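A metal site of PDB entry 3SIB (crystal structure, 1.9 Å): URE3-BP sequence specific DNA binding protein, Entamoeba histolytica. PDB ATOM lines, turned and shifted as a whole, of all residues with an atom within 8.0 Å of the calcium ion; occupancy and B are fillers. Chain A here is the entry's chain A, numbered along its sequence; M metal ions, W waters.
N of Phe 100 sits close to OD1 of Asp 97 (3.4 Å). The backbone NH of Gly 102 sits at hydrogen-bond distance from the side-chain carboxylate of Asp 97. The backbone NH of Glu 108 sits at hydrogen-bond distance from the side-chain hydroxyl of Ser 105, 3.1 Å away. The side-chain carboxylate (OE2) of Glu 108 sits close to the backbone NH (N) of Thr 98, at 3.2 Å.
The nearest printed residue that does not touch the calcium ion is Ile 104 (4.4 Å).
The calcium ion is bound by the side-chain carboxylate (OD1) of Asp 97 (2.2 Å), the backbone carbonyl oxygen (O) of His 103 (2.3 Å), the side-chain carboxylate (OD1) of Asp 99 (2.3 Å), water W1 (2.4 Å), the side-chain amide oxygen (OD1) of Asn 101 (2.5 Å), the side-chain carboxylate (OE1) of Glu 108 (2.6 Å) and the side-chain carboxylate (OE2) of Glu 108 (2.7 Å).
Water W1 bridges the side-chain carboxylate (OD2) of Asp 99 (2.9 Å) and the side-chain amide nitrogen (ND2) of Asn 101 (3.3 Å).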
ATOM      1  N   SER A  32      14.677  -7.045  24.735  1.00  0.00           N
ATOM      2  CA  SER A  32      14.619  -6.214  23.536  1.00  0.00           C
ATOM      3  C   SER A  32      15.639  -5.062  23.583  1.00  0.00           C
ATOM      4  O   SER A  32      16.149  -4.670  22.533  1.00  0.00           O
ATOM      5  CB  SER A  32      13.211  -5.636  23.342  1.00  0.00           C
ATOM      6  OG  SER A  32      12.840  -4.811  24.443  1.00  0.00           O
ATOM      7  N   VAL A  33      15.928  -4.536  24.761  1.00  0.00           N
ATOM      8  CA  VAL A  33      16.859  -3.435  24.924  1.00  0.00           C
ATOM      9  C   VAL A  33      18.291  -3.981  25.095  1.00  0.00           C
ATOM     10  O   VAL A  33      19.247  -3.453  24.519  1.00  0.00           O
ATOM     11  CB  VAL A  33      16.456  -2.538  26.136  1.00  0.00           C
ATOM     12  CG1 VAL A  33      17.580  -1.601  26.510  1.00  0.00           C
ATOM     13  CG2 VAL A  33      15.116  -1.746  25.821  1.00  0.00           C
ATOM     14  N   THR A  67       5.263   7.002  27.356  1.00  0.00           N
ATOM     15  CA  THR A  67       5.885   6.486  26.159  1.00  0.00           C
ATOM     16  C   THR A  67       5.958   7.603  25.090  1.00  0.00           C
ATOM     17  O   THR A  67       5.136   8.535  25.088  1.00  0.00           O
ATOM     18  CB  THR A  67       5.065   5.315  25.564  1.00  0.00           C
ATOM     19  OG1 THR A  67       3.749   5.785  25.219  1.00  0.00           O
ATOM     20  CG2 THR A  67       4.949   4.104  26.568  1.00  0.00           C
ATOM     21  N   LEU A  68       6.930   7.534  24.179  1.00  0.00           N
ATOM     22  CA  LEU A  68       7.006   8.502  23.079  1.00  0.00           C
ATOM     23  C   LEU A  68       6.485   7.901  21.802  1.00  0.00           C
ATOM     24  O   LEU A  68       6.861   6.778  21.408  1.00  0.00           O
ATOM     25  CB  LEU A  68       8.428   9.063  22.836  1.00  0.00           C
ATOM     26  CG  LEU A  68       9.177   9.505  24.100  1.00  0.00           C
ATOM     27  CD1 LEU A  68      10.530  10.088  23.691  1.00  0.00           C
ATOM     28  CD2 LEU A  68       8.345  10.501  24.898  1.00  0.00           C
ATOM     29  N   MET A  93      12.540   5.857  15.388  1.00  0.00           N
ATOM     30  CA  MET A  93      11.678   4.769  15.781  1.00  0.00           C
ATOM     31  C   MET A  93      12.269   3.427  15.363  1.00  0.00           C
ATOM     32  O   MET A  93      12.359   2.542  16.221  1.00  0.00           O
ATOM     33  CB  MET A  93      10.317   4.881  15.147  1.00  0.00           C
ATOM     34  CG  MET A  93       9.512   6.071  15.575  1.00  0.00           C
ATOM     35  SD  MET A  93       8.981   6.057  17.314  1.00  0.00           S
ATOM     36  CE  MET A  93       8.640   4.268  17.592  1.00  0.00           C
ATOM     37  N   PHE A  96      15.449   2.513  17.580  1.00  0.00           N
ATOM     38  CA  PHE A  96      15.327   2.433  19.039  1.00  0.00           C
ATOM     39  C   PHE A  96      14.078   1.714  19.555  1.00  0.00           C
ATOM     40  O   PHE A  96      14.063   1.279  20.703  1.00  0.00           O
ATOM     41  CB  PHE A  96      15.506   3.832  19.653  1.00  0.00           C
ATOM     42  CG  PHE A  96      16.911   4.386  19.451  1.00  0.00           C
ATOM     43  CD1 PHE A  96      17.989   3.830  20.145  1.00  0.00           C
ATOM     44  CD2 PHE A  96      17.162   5.387  18.527  1.00  0.00           C
ATOM     45  CE1 PHE A  96      19.305   4.280  19.901  1.00  0.00           C
ATOM     46  CE2 PHE A  96      18.470   5.834  18.288  1.00  0.00           C
ATOM     47  CZ  PHE A  96      19.524   5.322  19.006  1.00  0.00           C
ATOM     48  N   ASP A  97      13.077   1.534  18.713  1.00  0.00           N
ATOM     49  CA  ASP A  97      11.876   0.743  19.089  1.00  0.00           C
ATOM     50  C   ASP A  97      12.127  -0.731  18.885  1.00  0.00           C
ATOM     51  O   ASP A  97      11.663  -1.338  17.917  1.00  0.00           O
ATOM     52  CB  ASP A  97      10.644   1.183  18.295  1.00  0.00           C
ATOM     53  CG  ASP A  97       9.394   0.395  18.660  1.00  0.00           C
ATOM     54  OD1 ASP A  97       9.352  -0.152  19.790  1.00  0.00           O
ATOM     55  OD2 ASP A  97       8.464   0.365  17.825  1.00  0.00           O
ATOM     56  N   THR A  98      12.888  -1.326  19.778  1.00  0.00           N
ATOM     57  CA  THR A  98      13.416  -2.654  19.506  1.00  0.00           C
ATOM     58  C   THR A  98      12.507  -3.806  19.946  1.00  0.00           C
ATOM     59  O   THR A  98      12.882  -4.994  19.793  1.00  0.00           O
ATOM     60  CB  THR A  98      14.821  -2.824  20.051  1.00  0.00           C
ATOM     61  OG1 THR A  98      14.886  -2.405  21.418  1.00  0.00           O
ATOM     62  CG2 THR A  98      15.846  -1.967  19.202  1.00  0.00           C
ATOM     63  N   ASP A  99      11.358  -3.474  20.542  1.00  0.00           N
ATOM     64  CA  ASP A  99      10.289  -4.472  20.723  1.00  0.00           C
ATOM     65  C   ASP A  99       9.170  -4.292  19.702  1.00  0.00           C
ATOM     66  O   ASP A  99       8.146  -4.958  19.786  1.00  0.00           O
ATOM     67  CB  ASP A  99       9.735  -4.465  22.170  1.00  0.00           C
ATOM     68  CG  ASP A  99       9.205  -3.121  22.617  1.00  0.00           C
ATOM     69  OD1 ASP A  99       9.146  -2.161  21.816  1.00  0.00           O
ATOM     70  OD2 ASP A  99       8.832  -3.002  23.804  1.00  0.00           O
ATOM     71  N   PHE A 100       9.397  -3.412  18.726  1.00  0.00           N
ATOM     72  CA  PHE A 100       8.504  -3.220  17.563  1.00  0.00           C
ATOM     73  C   PHE A 100       7.046  -2.942  17.970  1.00  0.00           C
ATOM     74  O   PHE A 100       6.105  -3.507  17.389  1.00  0.00           O
ATOM     75  CB  PHE A 100       8.597  -4.394  16.553  1.00  0.00           C
ATOM     76  CG  PHE A 100      10.022  -4.851  16.262  1.00  0.00           C
ATOM     77  CD1 PHE A 100      10.789  -4.219  15.281  1.00  0.00           C
ATOM     78  CD2 PHE A 100      10.601  -5.895  16.970  1.00  0.00           C
ATOM     79  CE1 PHE A 100      12.111  -4.630  15.030  1.00  0.00           C
ATOM     80  CE2 PHE A 100      11.925  -6.310  16.702  1.00  0.00           C
ATOM     81  CZ  PHE A 100      12.670  -5.671  15.729  1.00  0.00           C
ATOM     82  N   ASN A 101       6.847  -2.087  18.984  1.00  0.00           N
ATOM     83  CA  ASN A 101       5.484  -1.801  19.434  1.00  0.00           C
ATOM     84  C   ASN A 101       4.981  -0.417  19.065  1.00  0.00           C
ATOM     85  O   ASN A 101       3.878  -0.038  19.470  1.00  0.00           O
ATOM     86  CB  ASN A 101       5.307  -2.079  20.953  1.00  0.00           C
ATOM     87  CG  ASN A 101       5.994  -1.071  21.829  1.00  0.00           C
ATOM     88  OD1 ASN A 101       6.825  -0.285  21.378  1.00  0.00           O
ATOM     89  ND2 ASN A 101       5.652  -1.094  23.130  1.00  0.00           N
ATOM     90  N   GLY A 102       5.782   0.345  18.325  1.00  0.00           N
ATOM     91  CA  GLY A 102       5.359   1.664  17.859  1.00  0.00           C
ATOM     92  C   GLY A 102       5.423   2.720  18.934  1.00  0.00           C
ATOM     93  O   GLY A 102       4.887   3.816  18.766  1.00  0.00           O
ATOM     94  N   HIS A 103       6.123   2.417  20.034  1.00  0.00           N
ATOM     95  CA  HIS A 103       6.264   3.361  21.125  1.00  0.00           C
ATOM     96  C   HIS A 103       7.718   3.317  21.603  1.00  0.00           C
ATOM     97  O   HIS A 103       8.364   2.255  21.589  1.00  0.00           O
ATOM     98  CB  HIS A 103       5.330   3.043  22.303  1.00  0.00           C
ATOM     99  CG  HIS A 103       3.877   2.986  21.967  1.00  0.00           C
ATOM    100  ND1 HIS A 103       3.054   4.097  21.977  1.00  0.00           N
ATOM    101  CD2 HIS A 103       3.094   1.942  21.596  1.00  0.00           C
ATOM    102  CE1 HIS A 103       1.828   3.734  21.644  1.00  0.00           C
ATOM    103  NE2 HIS A 103       1.817   2.427  21.430  1.00  0.00           N
ATOM    104  N   ILE A 104       8.260   4.469  21.981  1.00  0.00           N
ATOM    105  CA  ILE A 104       9.604   4.546  22.575  1.00  0.00           C
ATOM    106  C   ILE A 104       9.443   4.590  24.074  1.00  0.00           C
ATOM    107  O   ILE A 104       8.898   5.545  24.599  1.00  0.00           O
ATOM    108  CB  ILE A 104      10.377   5.785  22.067  1.00  0.00           C
ATOM    109  CG1 ILE A 104      10.672   5.645  20.579  1.00  0.00           C
ATOM    110  CG2 ILE A 104      11.712   6.050  22.837  1.00  0.00           C
ATOM    111  CD1 ILE A 104      11.623   4.577  20.261  1.00  0.00           C
ATOM    112  N   SER A 105       9.934   3.550  24.737  1.00  0.00           N
ATOM    113  CA  SER A 105       9.960   3.482  26.207  1.00  0.00           C
ATOM    114  C   SER A 105      11.044   4.369  26.780  1.00  0.00           C
ATOM    115  O   SER A 105      11.902   4.862  26.042  1.00  0.00           O
ATOM    116  CB  SER A 105      10.263   2.052  26.670  1.00  0.00           C
ATOM    117  OG  SER A 105      11.631   1.742  26.387  1.00  0.00           O
ATOM    118  N   PHE A 106      11.021   4.590  28.096  1.00  0.00           N
ATOM    119  CA  PHE A 106      12.097   5.384  28.683  1.00  0.00           C
ATOM    120  C   PHE A 106      13.479   4.804  28.399  1.00  0.00           C
ATOM    121  O   PHE A 106      14.401   5.547  28.115  1.00  0.00           O
ATOM    122  CB  PHE A 106      11.957   5.600  30.185  1.00  0.00           C
ATOM    123  CG  PHE A 106      13.090   6.418  30.772  1.00  0.00           C
ATOM    124  CD1 PHE A 106      13.309   7.701  30.345  1.00  0.00           C
ATOM    125  CD2 PHE A 106      13.913   5.894  31.762  1.00  0.00           C
ATOM    126  CE1 PHE A 106      14.380   8.453  30.822  1.00  0.00           C
ATOM    127  CE2 PHE A 106      14.952   6.658  32.288  1.00  0.00           C
ATOM    128  CZ  PHE A 106      15.190   7.929  31.811  1.00  0.00           C
ATOM    129  N   GLU A 108      14.490   2.884  25.827  1.00  0.00           N
ATOM    130  CA  GLU A 108      14.813   3.101  24.419  1.00  0.00           C
ATOM    131  C   GLU A 108      15.205   4.575  24.201  1.00  0.00           C
ATOM    132  O   GLU A 108      16.101   4.888  23.432  1.00  0.00           O
ATOM    133  CB  GLU A 108      13.609   2.712  23.541  1.00  0.00           C
ATOM    134  CG  GLU A 108      13.294   1.190  23.617  1.00  0.00           C
ATOM    135  CD  GLU A 108      11.961   0.805  22.981  1.00  0.00           C
ATOM    136  OE1 GLU A 108      11.047   1.661  22.893  1.00  0.00           O
ATOM    137  OE2 GLU A 108      11.809  -0.400  22.611  1.00  0.00           O
HETATM  138 CA    CA M   1       9.190   0.143  21.998  1.00  0.00          CA
HETATM  139  O   HOH W   1       8.603  -0.126  24.333  1.00  0.00           O
